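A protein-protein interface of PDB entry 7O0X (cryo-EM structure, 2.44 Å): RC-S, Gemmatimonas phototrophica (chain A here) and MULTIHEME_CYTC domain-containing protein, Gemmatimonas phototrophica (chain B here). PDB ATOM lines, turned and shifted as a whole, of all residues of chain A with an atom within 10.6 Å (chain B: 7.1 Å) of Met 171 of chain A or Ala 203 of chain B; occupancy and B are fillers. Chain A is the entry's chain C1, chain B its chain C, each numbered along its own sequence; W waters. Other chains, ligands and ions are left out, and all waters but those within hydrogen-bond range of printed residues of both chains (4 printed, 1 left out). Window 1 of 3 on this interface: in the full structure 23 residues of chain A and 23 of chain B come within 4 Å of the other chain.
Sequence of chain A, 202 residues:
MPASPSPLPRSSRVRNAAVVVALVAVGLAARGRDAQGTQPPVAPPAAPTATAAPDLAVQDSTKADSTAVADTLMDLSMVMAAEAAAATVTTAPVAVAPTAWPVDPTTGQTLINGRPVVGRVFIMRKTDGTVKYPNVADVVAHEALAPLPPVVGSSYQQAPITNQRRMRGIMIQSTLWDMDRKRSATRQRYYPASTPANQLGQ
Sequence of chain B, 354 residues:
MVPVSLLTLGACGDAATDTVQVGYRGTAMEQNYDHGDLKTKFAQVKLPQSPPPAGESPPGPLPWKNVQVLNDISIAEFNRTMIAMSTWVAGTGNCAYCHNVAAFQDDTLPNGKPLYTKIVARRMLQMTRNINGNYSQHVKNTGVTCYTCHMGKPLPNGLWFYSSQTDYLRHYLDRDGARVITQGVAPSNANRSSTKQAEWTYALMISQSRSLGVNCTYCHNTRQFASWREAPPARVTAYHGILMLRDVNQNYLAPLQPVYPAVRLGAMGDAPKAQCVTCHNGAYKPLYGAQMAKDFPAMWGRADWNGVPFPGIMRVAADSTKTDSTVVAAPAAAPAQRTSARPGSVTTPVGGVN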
ATOM      1  N   ARG A 165       7.058  38.154 -11.818  1.00  0.00           N
ATOM      2  CA  ARG A 165       6.663  36.916 -11.158  1.00  0.00           C
ATOM      3  C   ARG A 165       7.599  36.632  -9.994  1.00  0.00           C
ATOM      4  O   ARG A 165       8.821  36.732 -10.128  1.00  0.00           O
ATOM      5  CB  ARG A 165       6.745  35.742 -12.131  1.00  0.00           C
ATOM      6  CG  ARG A 165       5.785  35.733 -13.296  1.00  0.00           C
ATOM      7  CD  ARG A 165       6.018  34.454 -14.087  1.00  0.00           C
ATOM      8  NE  ARG A 165       5.238  34.383 -15.313  1.00  0.00           N
ATOM      9  CZ  ARG A 165       5.124  33.296 -16.064  1.00  0.00           C
ATOM     10  NH1 ARG A 165       5.837  32.209 -15.818  1.00  0.00           N
ATOM     11  NH2 ARG A 165       4.313  33.317 -17.117  1.00  0.00           N
ATOM     12  N   MET A 167       7.448  33.533  -8.586  1.00  0.00           N
ATOM     13  CA  MET A 167       7.870  32.180  -8.942  1.00  0.00           C
ATOM     14  C   MET A 167       8.690  32.220 -10.228  1.00  0.00           C
ATOM     15  O   MET A 167       8.193  32.649 -11.274  1.00  0.00           O
ATOM     16  CB  MET A 167       6.673  31.246  -9.080  1.00  0.00           C
ATOM     17  CG  MET A 167       6.082  30.859  -7.736  1.00  0.00           C
ATOM     18  SD  MET A 167       4.700  29.716  -7.837  1.00  0.00           S
ATOM     19  CE  MET A 167       5.586  28.195  -8.150  1.00  0.00           C
ATOM     20  N   ARG A 168       9.943  31.771 -10.148  1.00  0.00           N
ATOM     21  CA  ARG A 168      10.856  31.776 -11.284  1.00  0.00           C
ATOM     22  C   ARG A 168      10.859  30.480 -12.092  1.00  0.00           C
ATOM     23  O   ARG A 168      11.522  30.430 -13.133  1.00  0.00           O
ATOM     24  CB  ARG A 168      12.277  32.103 -10.810  1.00  0.00           C
ATOM     25  CG  ARG A 168      12.393  33.513 -10.250  1.00  0.00           C
ATOM     26  CD  ARG A 168      13.799  33.867  -9.797  1.00  0.00           C
ATOM     27  NE  ARG A 168      14.774  33.734 -10.871  1.00  0.00           N
ATOM     28  CZ  ARG A 168      15.737  32.824 -10.910  1.00  0.00           C
ATOM     29  NH1 ARG A 168      15.985  32.037  -9.877  1.00  0.00           N
ATOM     30  NH2 ARG A 168      16.505  32.738 -11.991  1.00  0.00           N
ATOM     31  N   GLY A 169      10.167  29.434 -11.642  1.00  0.00           N
ATOM     32  CA  GLY A 169      10.081  28.202 -12.411  1.00  0.00           C
ATOM     33  C   GLY A 169       9.453  28.409 -13.778  1.00  0.00           C
ATOM     34  O   GLY A 169       8.414  29.063 -13.894  1.00  0.00           O
ATOM     35  N   ILE A 170      10.082  27.862 -14.821  1.00  0.00           N
ATOM     36  CA  ILE A 170       9.737  28.249 -16.188  1.00  0.00           C
ATOM     37  C   ILE A 170       8.425  27.627 -16.681  1.00  0.00           C
ATOM     38  O   ILE A 170       7.715  28.243 -17.483  1.00  0.00           O
ATOM     39  CB  ILE A 170      10.904  27.892 -17.130  1.00  0.00           C
ATOM     40  CG1 ILE A 170      12.188  28.614 -16.714  1.00  0.00           C
ATOM     41  CG2 ILE A 170      10.574  28.243 -18.571  1.00  0.00           C
ATOM     42  CD1 ILE A 170      12.063  30.119 -16.662  1.00  0.00           C
ATOM     43  N   MET A 171       8.051  26.440 -16.209  1.00  0.00           N
ATOM     44  CA  MET A 171       6.852  25.780 -16.720  1.00  0.00           C
ATOM     45  C   MET A 171       5.598  26.025 -15.888  1.00  0.00           C
ATOM     46  O   MET A 171       4.547  25.462 -16.208  1.00  0.00           O
ATOM     47  CB  MET A 171       7.094  24.274 -16.861  1.00  0.00           C
ATOM     48  CG  MET A 171       8.196  23.933 -17.851  1.00  0.00           C
ATOM     49  SD  MET A 171       8.299  22.183 -18.254  1.00  0.00           S
ATOM     50  CE  MET A 171       6.709  21.930 -19.034  1.00  0.00           C
ATOM     51  N   ILE A 172       5.684  26.839 -14.834  1.00  0.00           N
ATOM     52  CA  ILE A 172       4.610  26.951 -13.848  1.00  0.00           C
ATOM     53  C   ILE A 172       3.292  27.411 -14.470  1.00  0.00           C
ATOM     54  O   ILE A 172       2.211  27.015 -14.015  1.00  0.00           O
ATOM     55  CB  ILE A 172       5.054  27.878 -12.696  1.00  0.00           C
ATOM     56  CG1 ILE A 172       4.128  27.702 -11.495  1.00  0.00           C
ATOM     57  CG2 ILE A 172       5.119  29.333 -13.143  1.00  0.00           C
ATOM     58  CD1 ILE A 172       4.289  26.365 -10.822  1.00  0.00           C
ATOM     59  N   GLN A 173       3.354  28.245 -15.509  1.00  0.00           N
ATOM     60  CA  GLN A 173       2.145  28.722 -16.177  1.00  0.00           C
ATOM     61  C   GLN A 173       1.326  27.587 -16.788  1.00  0.00           C
ATOM     62  O   GLN A 173       0.091  27.618 -16.743  1.00  0.00           O
ATOM     63  CB  GLN A 173       2.523  29.765 -17.231  1.00  0.00           C
ATOM     64  CG  GLN A 173       1.355  30.419 -17.946  1.00  0.00           C
ATOM     65  CD  GLN A 173       1.804  31.439 -18.975  1.00  0.00           C
ATOM     66  OE1 GLN A 173       2.996  31.702 -19.127  1.00  0.00           O
ATOM     67  NE2 GLN A 173       0.846  32.022 -19.687  1.00  0.00           N
ATOM     68  N   SER A 174       1.979  26.571 -17.354  1.00  0.00           N
ATOM     69  CA  SER A 174       1.241  25.415 -17.856  1.00  0.00           C
ATOM     70  C   SER A 174       1.049  24.299 -16.834  1.00  0.00           C
ATOM     71  O   SER A 174       0.001  23.647 -16.833  1.00  0.00           O
ATOM     72  CB  SER A 174       1.935  24.838 -19.092  1.00  0.00           C
ATOM     73  OG  SER A 174       1.989  25.788 -20.137  1.00  0.00           O
ATOM     74  N   THR A 175       2.028  24.051 -15.966  1.00  0.00           N
ATOM     75  CA  THR A 175       1.923  22.903 -15.072  1.00  0.00           C
ATOM     76  C   THR A 175       1.030  23.170 -13.866  1.00  0.00           C
ATOM     77  O   THR A 175       0.379  22.243 -13.374  1.00  0.00           O
ATOM     78  CB  THR A 175       3.310  22.456 -14.605  1.00  0.00           C
ATOM     79  OG1 THR A 175       3.999  23.558 -14.001  1.00  0.00           O
ATOM     80  CG2 THR A 175       4.121  21.932 -15.780  1.00  0.00           C
ATOM     81  N   LEU A 176       0.976  24.406 -13.374  1.00  0.00           N
ATOM     82  CA  LEU A 176       0.105  24.729 -12.250  1.00  0.00           C
ATOM     83  C   LEU A 176      -0.972  25.746 -12.589  1.00  0.00           C
ATOM     84  O   LEU A 176      -2.156  25.482 -12.355  1.00  0.00           O
ATOM     85  CB  LEU A 176       0.942  25.225 -11.064  1.00  0.00           C
ATOM     86  CG  LEU A 176       0.165  25.552  -9.790  1.00  0.00           C
ATOM     87  CD1 LEU A 176      -0.526  24.309  -9.276  1.00  0.00           C
ATOM     88  CD2 LEU A 176       1.094  26.110  -8.733  1.00  0.00           C
ATOM     89  N   TRP A 177      -0.601  26.915 -13.120  1.00  0.00           N
ATOM     90  CA  TRP A 177      -1.517  28.053 -13.111  1.00  0.00           C
ATOM     91  C   TRP A 177      -2.719  27.857 -14.025  1.00  0.00           C
ATOM     92  O   TRP A 177      -3.790  28.409 -13.753  1.00  0.00           O
ATOM     93  CB  TRP A 177      -0.790  29.343 -13.498  1.00  0.00           C
ATOM     94  CG  TRP A 177       0.246  29.793 -12.522  1.00  0.00           C
ATOM     95  CD1 TRP A 177       0.510  29.252 -11.301  1.00  0.00           C
ATOM     96  CD2 TRP A 177       1.119  30.921 -12.659  1.00  0.00           C
ATOM     97  NE1 TRP A 177       1.511  29.956 -10.678  1.00  0.00           N
ATOM     98  CE2 TRP A 177       1.900  30.987 -11.491  1.00  0.00           C
ATOM     99  CE3 TRP A 177       1.321  31.875 -13.661  1.00  0.00           C
ATOM    100  CZ2 TRP A 177       2.870  31.967 -11.297  1.00  0.00           C
ATOM    101  CZ3 TRP A 177       2.284  32.846 -13.468  1.00  0.00           C
ATOM    102  CH2 TRP A 177       3.047  32.886 -12.295  1.00  0.00           C
ATOM    103  N   ASP A 178      -2.578  27.086 -15.102  1.00  0.00           N
ATOM    104  CA  ASP A 178      -3.713  26.864 -15.990  1.00  0.00           C
ATOM    105  C   ASP A 178      -4.821  26.023 -15.365  1.00  0.00           C
ATOM    106  O   ASP A 178      -5.964  26.101 -15.827  1.00  0.00           O
ATOM    107  CB  ASP A 178      -3.240  26.220 -17.294  1.00  0.00           C
ATOM    108  CG  ASP A 178      -2.576  27.216 -18.225  1.00  0.00           C
ATOM    109  OD1 ASP A 178      -2.836  28.430 -18.079  1.00  0.00           O
ATOM    110  OD2 ASP A 178      -1.801  26.790 -19.105  1.00  0.00           O
ATOM    111  N   MET A 179      -4.528  25.225 -14.342  1.00  0.00           N
ATOM    112  CA  MET A 179      -5.580  24.561 -13.579  1.00  0.00           C
ATOM    113  C   MET A 179      -5.917  25.230 -12.248  1.00  0.00           C
ATOM    114  O   MET A 179      -7.059  25.117 -11.791  1.00  0.00           O
ATOM    115  CB  MET A 179      -5.221  23.084 -13.366  1.00  0.00           C
ATOM    116  CG  MET A 179      -4.053  22.794 -12.446  1.00  0.00           C
ATOM    117  SD  MET A 179      -3.844  21.009 -12.265  1.00  0.00           S
ATOM    118  CE  MET A 179      -2.372  20.923 -11.256  1.00  0.00           C
ATOM    119  N   ASP A 180      -4.970  25.914 -11.608  1.00  0.00           N
ATOM    120  CA  ASP A 180      -5.192  26.526 -10.296  1.00  0.00           C
ATOM    121  C   ASP A 180      -5.926  27.860 -10.432  1.00  0.00           C
ATOM    122  O   ASP A 180      -5.385  28.818 -10.994  1.00  0.00           O
ATOM    123  CB  ASP A 180      -3.857  26.719  -9.583  1.00  0.00           C
ATOM    124  CG  ASP A 180      -4.019  27.272  -8.185  1.00  0.00           C
ATOM    125  OD1 ASP A 180      -5.072  27.024  -7.563  1.00  0.00           O
ATOM    126  OD2 ASP A 180      -3.092  27.953  -7.705  1.00  0.00           O
ATOM    127  N   TYR B 168       4.153  32.920 -22.244  1.00  0.00           N
ATOM    128  CA  TYR B 168       4.338  32.288 -23.548  1.00  0.00           C
ATOM    129  C   TYR B 168       3.270  32.666 -24.568  1.00  0.00           C
ATOM    130  O   TYR B 168       3.488  32.463 -25.766  1.00  0.00           O
ATOM    131  CB  TYR B 168       4.416  30.761 -23.420  1.00  0.00           C
ATOM    132  CG  TYR B 168       3.254  30.072 -22.735  1.00  0.00           C
ATOM    133  CD1 TYR B 168       1.989  30.039 -23.309  1.00  0.00           C
ATOM    134  CD2 TYR B 168       3.444  29.395 -21.541  1.00  0.00           C
ATOM    135  CE1 TYR B 168       0.931  29.434 -22.664  1.00  0.00           C
ATOM    136  CE2 TYR B 168       2.403  28.749 -20.914  1.00  0.00           C
ATOM    137  CZ  TYR B 168       1.146  28.781 -21.470  1.00  0.00           C
ATOM    138  OH  TYR B 168       0.123  28.098 -20.863  1.00  0.00           O
ATOM    139  N   LYS B 196      16.486  26.237 -20.060  1.00  0.00           N
ATOM    140  CA  LYS B 196      15.328  27.044 -19.680  1.00  0.00           C
ATOM    141  C   LYS B 196      14.467  27.420 -20.879  1.00  0.00           C
ATOM    142  O   LYS B 196      13.238  27.484 -20.771  1.00  0.00           O
ATOM    143  CB  LYS B 196      15.791  28.308 -18.960  1.00  0.00           C
ATOM    144  CG  LYS B 196      16.445  28.074 -17.620  1.00  0.00           C
ATOM    145  CD  LYS B 196      16.809  29.398 -16.983  1.00  0.00           C
ATOM    146  CE  LYS B 196      17.484  29.203 -15.643  1.00  0.00           C
ATOM    147  NZ  LYS B 196      16.685  29.812 -14.553  1.00  0.00           N
ATOM    148  N   GLN B 197      15.088  27.684 -22.025  1.00  0.00           N
ATOM    149  CA  GLN B 197      14.320  27.972 -23.231  1.00  0.00           C
ATOM    150  C   GLN B 197      13.563  26.745 -23.728  1.00  0.00           C
ATOM    151  O   GLN B 197      12.437  26.866 -24.222  1.00  0.00           O
ATOM    152  CB  GLN B 197      15.242  28.533 -24.311  1.00  0.00           C
ATOM    153  CG  GLN B 197      15.730  29.936 -23.992  1.00  0.00           C
ATOM    154  CD  GLN B 197      16.719  30.461 -25.003  1.00  0.00           C
ATOM    155  OE1 GLN B 197      17.801  29.907 -25.169  1.00  0.00           O
ATOM    156  NE2 GLN B 197      16.357  31.539 -25.684  1.00  0.00           N
ATOM    157  N   ALA B 198      14.160  25.559 -23.605  1.00  0.00           N
ATOM    158  CA  ALA B 198      13.430  24.327 -23.888  1.00  0.00           C
ATOM    159  C   ALA B 198      12.268  24.112 -22.922  1.00  0.00           C
ATOM    160  O   ALA B 198      11.214  23.605 -23.322  1.00  0.00           O
ATOM    161  CB  ALA B 198      14.385  23.135 -23.850  1.00  0.00           C
ATOM    162  N   GLU B 199      12.433  24.482 -21.649  1.00  0.00           N
ATOM    163  CA  GLU B 199      11.294  24.488 -20.732  1.00  0.00           C
ATOM    164  C   GLU B 199      10.206  25.456 -21.178  1.00  0.00           C
ATOM    165  O   GLU B 199       9.013  25.161 -21.047  1.00  0.00           O
ATOM    166  CB  GLU B 199      11.743  24.829 -19.309  1.00  0.00           C
ATOM    167  CG  GLU B 199      12.611  23.778 -18.656  1.00  0.00           C
ATOM    168  CD  GLU B 199      13.105  24.171 -17.281  1.00  0.00           C
ATOM    169  OE1 GLU B 199      12.345  23.994 -16.306  1.00  0.00           O
ATOM    170  OE2 GLU B 199      14.257  24.636 -17.169  1.00  0.00           O
ATOM    171  N   TRP B 200      10.593  26.619 -21.705  1.00  0.00           N
ATOM    172  CA  TRP B 200       9.607  27.592 -22.164  1.00  0.00           C
ATOM    173  C   TRP B 200       8.839  27.091 -23.383  1.00  0.00           C
ATOM    174  O   TRP B 200       7.615  27.249 -23.456  1.00  0.00           O
ATOM    175  CB  TRP B 200      10.302  28.917 -22.468  1.00  0.00           C
ATOM    176  CG  TRP B 200       9.388  30.038 -22.855  1.00  0.00           C
ATOM    177  CD1 TRP B 200       8.833  30.960 -22.019  1.00  0.00           C
ATOM    178  CD2 TRP B 200       8.938  30.372 -24.174  1.00  0.00           C
ATOM    179  NE1 TRP B 200       8.058  31.840 -22.730  1.00  0.00           N
ATOM    180  CE2 TRP B 200       8.107  31.502 -24.056  1.00  0.00           C
ATOM    181  CE3 TRP B 200       9.154  29.824 -25.442  1.00  0.00           C
ATOM    182  CZ2 TRP B 200       7.491  32.094 -25.156  1.00  0.00           C
ATOM    183  CZ3 TRP B 200       8.539  30.412 -26.532  1.00  0.00           C
ATOM    184  CH2 TRP B 200       7.718  31.535 -26.382  1.00  0.00           C
ATOM    185  N   THR B 201       9.536  26.494 -24.351  1.00  0.00           N
ATOM    186  CA  THR B 201       8.857  25.879 -25.489  1.00  0.00           C
ATOM    187  C   THR B 201       7.952  24.735 -25.047  1.00  0.00           C
ATOM    188  O   THR B 201       6.848  24.566 -25.575  1.00  0.00           O
ATOM    189  CB  THR B 201       9.884  25.389 -26.511  1.00  0.00           C
ATOM    190  OG1 THR B 201      10.640  26.502 -26.997  1.00  0.00           O
ATOM    191  CG2 THR B 201       9.196  24.719 -27.689  1.00  0.00           C
ATOM    192  N   TYR B 202       8.405  23.941 -24.076  1.00  0.00           N
ATOM    193  CA  TYR B 202       7.594  22.847 -23.554  1.00  0.00           C
ATOM    194  C   TYR B 202       6.297  23.357 -22.931  1.00  0.00           C
ATOM    195  O   TYR B 202       5.224  22.792 -23.170  1.00  0.00           O
ATOM    196  CB  TYR B 202       8.429  22.062 -22.538  1.00  0.00           C
ATOM    197  CG  TYR B 202       7.925  20.693 -22.136  1.00  0.00           C
ATOM    198  CD1 TYR B 202       6.772  20.149 -22.681  1.00  0.00           C
ATOM    199  CD2 TYR B 202       8.641  19.924 -21.230  1.00  0.00           C
ATOM    200  CE1 TYR B 202       6.332  18.893 -22.306  1.00  0.00           C
ATOM    201  CE2 TYR B 202       8.214  18.671 -20.856  1.00  0.00           C
ATOM    202  CZ  TYR B 202       7.061  18.159 -21.397  1.00  0.00           C
ATOM    203  OH  TYR B 202       6.637  16.907 -21.021  1.00  0.00           O
ATOM    204  N   ALA B 203       6.374  24.425 -22.133  1.00  0.00           N
ATOM    205  CA  ALA B 203       5.169  25.050 -21.591  1.00  0.00           C
ATOM    206  C   ALA B 203       4.232  25.534 -22.694  1.00  0.00           C
ATOM    207  O   ALA B 203       3.022  25.285 -22.651  1.00  0.00           O
ATOM    208  CB  ALA B 203       5.553  26.208 -20.670  1.00  0.00           C
ATOM    209  N   LEU B 204       4.780  26.235 -23.690  1.00  0.00           N
ATOM    210  CA  LEU B 204       4.002  26.655 -24.854  1.00  0.00           C
ATOM    211  C   LEU B 204       3.328  25.483 -25.560  1.00  0.00           C
ATOM    212  O   LEU B 204       2.171  25.588 -25.982  1.00  0.00           O
ATOM    213  CB  LEU B 204       4.909  27.408 -25.826  1.00  0.00           C
ATOM    214  CG  LEU B 204       4.328  27.793 -27.186  1.00  0.00           C
ATOM    215  CD1 LEU B 204       3.288  28.887 -27.040  1.00  0.00           C
ATOM    216  CD2 LEU B 204       5.438  28.224 -28.124  1.00  0.00           C
ATOM    217  N   MET B 205       4.031  24.362 -25.702  1.00  0.00           N
ATOM    218  CA  MET B 205       3.508  23.228 -26.455  1.00  0.00           C
ATOM    219  C   MET B 205       2.442  22.449 -25.696  1.00  0.00           C
ATOM    220  O   MET B 205       1.526  21.902 -26.317  1.00  0.00           O
ATOM    221  CB  MET B 205       4.666  22.312 -26.848  1.00  0.00           C
ATOM    222  CG  MET B 205       5.532  22.908 -27.936  1.00  0.00           C
ATOM    223  SD  MET B 205       4.665  23.031 -29.510  1.00  0.00           S
ATOM    224  CE  MET B 205       5.438  24.498 -30.174  1.00  0.00           C
ATOM    225  N   ILE B 206       2.539  22.390 -24.369  1.00  0.00           N
ATOM    226  CA  ILE B 206       1.443  21.859 -23.562  1.00  0.00           C
ATOM    227  C   ILE B 206       0.170  22.671 -23.774  1.00  0.00           C
ATOM    228  O   ILE B 206      -0.921  22.112 -23.940  1.00  0.00           O
ATOM    229  CB  ILE B 206       1.852  21.811 -22.078  1.00  0.00           C
ATOM    230  CG1 ILE B 206       2.898  20.718 -21.855  1.00  0.00           C
ATOM    231  CG2 ILE B 206       0.648  21.563 -21.192  1.00  0.00           C
ATOM    232  CD1 ILE B 206       3.536  20.750 -20.489  1.00  0.00           C
ATOM    233  N   SER B 207       0.289  24.001 -23.787  1.00  0.00           N
ATOM    234  CA  SER B 207      -0.855  24.866 -24.066  1.00  0.00           C
ATOM    235  C   SER B 207      -1.494  24.592 -25.427  1.00  0.00           C
ATOM    236  O   SER B 207      -2.723  24.533 -25.534  1.00  0.00           O
ATOM    237  CB  SER B 207      -0.423  26.329 -23.974  1.00  0.00           C
ATOM    238  OG  SER B 207      -1.529  27.195 -24.137  1.00  0.00           O
ATOM    239  N   GLN B 208      -0.690  24.421 -26.477  1.00  0.00           N
ATOM    240  CA  GLN B 208      -1.257  24.082 -27.781  1.00  0.00           C
ATOM    241  C   GLN B 208      -1.922  22.710 -27.784  1.00  0.00           C
ATOM    242  O   GLN B 208      -2.982  22.532 -28.396  1.00  0.00           O
ATOM    243  CB  GLN B 208      -0.184  24.155 -28.866  1.00  0.00           C
ATOM    244  CG  GLN B 208       0.317  25.558 -29.132  1.00  0.00           C
ATOM    245  CD  GLN B 208       1.250  25.632 -30.322  1.00  0.00           C
ATOM    246  OE1 GLN B 208       1.444  24.651 -31.037  1.00  0.00           O
ATOM    247  NE2 GLN B 208       1.834  26.802 -30.541  1.00  0.00           N
ATOM    248  N   ARG B 210      -3.358  21.128 -25.200  1.00  0.00           N
ATOM    249  CA  ARG B 210      -4.631  21.279 -24.503  1.00  0.00           C
ATOM    250  C   ARG B 210      -5.643  22.086 -25.308  1.00  0.00           C
ATOM    251  O   ARG B 210      -6.845  21.799 -25.263  1.00  0.00           O
ATOM    252  CB  ARG B 210      -4.391  21.934 -23.147  1.00  0.00           C
ATOM    253  CG  ARG B 210      -3.762  21.015 -22.121  1.00  0.00           C
ATOM    254  CD  ARG B 210      -3.486  21.768 -20.839  1.00  0.00           C
ATOM    255  NE  ARG B 210      -2.855  20.933 -19.825  1.00  0.00           N
ATOM    256  CZ  ARG B 210      -2.119  21.404 -18.828  1.00  0.00           C
ATOM    257  NH1 ARG B 210      -1.830  22.690 -18.732  1.00  0.00           N
ATOM    258  NH2 ARG B 210      -1.645  20.561 -17.918  1.00  0.00           N
HETATM  259  O   HOH W   1      12.405  26.190 -14.223  1.00  0.00           O
HETATM  260  O   HOH W   2      -2.459  25.077 -20.814  1.00  0.00           O
HETATM  261  O   HOH W   3      -1.930  29.758 -20.263  1.00  0.00           O
HETATM  262  O   HOH W   4      16.010  32.448 -15.407  1.00  0.00           O
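The side-chain hydroxyl (OH) of Tyr 168 of chain B lies within hydrogen-bond range of the side-chain hydroxyl (OG) of Ser 174 of chain A (3.1 Å). The side-chain hydroxyl of Tyr 168 of chain B lies within hydrogen-bond range of the side-chain carboxylate of Asp 178 of chain A, 2.9 Å away. The side-chain hydroxyl of Ser 174 of chain A is in hydrogen-bond range of the backbone carbonyl oxygen of Ala 203 of chain B (2.8 Å). The backbone carbonyl oxygen of Ser 174 of chain A lies within hydrogen-bond range of the guanidinium group of Arg 210 of chain B (2.8 Å).
The guanidinium group (NH2) of Arg 165 of chain A is in hydrogen-bond range of the side-chain amide oxygen (OE1) of Gln 173 of chain A, at 2.9 Å. The side-chain hydroxyl (OG1) of Thr 175 of chain A is in hydrogen-bond range of the backbone carbonyl oxygen (O) of Met 171 of chain A. The backbone carbonyl oxygen of Gln 173 of chain A sits close to the backbone NH of Asp 178 of chain A, at 3.2 Å.
Arg 168 of chain A touches Lys 196 of chain B. Lys 196 of chain B touches Ile 170 of chain A (O to CG2, 3.5 Å). CG2 of Ile 170 of chain A touches CB of Glu 199 of chain B (3.7 Å). CG2 of Ile 170 of chain A touches N of Trp 200 of chain B, at 3.5 Å. Met 171 of chain A touches Glu 199 of chain B (CG to O, 3.5 Å). Met 171 of chain A touches Tyr 202 of chain B (CE to CD2, 3.5 Å). Ala 203 of chain B touches Met 171 of chain A. Ile 206 of chain B touches Met 171 of chain A (CD1 to CE, 3.7 Å). OE1 of Gln 173 of chain A touches CD2 of Tyr 168 of chain B, at 3.4 Å.
Of the printed residues of chain B, Met 171 of chain A touches Glu 199, Tyr 202, Ala 203 and Ile 206. Of the printed residues of chain B, Gln 173 of chain A touches Tyr 168. Of the printed residues of chain B, Asp 178 of chain A touches Tyr 168. Of the printed residues of chain A, Tyr 168 of chain B touches Gln 173, Ser 174 and Asp 178. Glu 199 of chain B touches just these residues of chain A: Ile 170 and Met 171. Printed residues of chain A within 4 Å of Trp 200 of chain B: Ile 170. Printed residues of chain A within 4 Å of Ala 203 of chain B: Met 171 (3.99 Å) and Ser 174 (2.8 Å). No residue of chain A comes within 4 Å of Leu 204 of chain B. The nearest printed residue of chain B that does not touch Met 171 of chain A is Trp 200 of chain B (5.3 Å).
Hydrophobic or aromatic side chains of chain B that line the printed part of chain A: Tyr 168, Trp 200, Tyr 202, Ala 203 and Ile 206. Hydrophobic or aromatic side chains of chain A within 4 Å of the printed part of chain B: Ile 170 and Met 171. Among the printed residues, no Asp or Glu carboxylate lies within 4 Å of a Lys or Arg side-chain nitrogen of the other chain.
Water W2 bridges OD2 of Asp 178 of chain A and NH1 of Arg 210 of chain B. Water W3 lies within hydrogen-bond range of the side-chain hydroxyl (OH) of Tyr 168 of chain B (2.7 Å) and the side-chain carboxylate (OD1) of Asp 178 of chain A (2.7 Å). Water W4 bridges NZ of Lys 196 of chain B (2.9 Å) and NH2 of Arg 168 of chain A (3.5 Å). Water W1 lies within hydrogen-bond range of the backbone NH (N) of Ile 170 of chain A (2.9 Å) and the side-chain carboxylate (OE1) of Glu 199 of chain B (3.0 Å).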
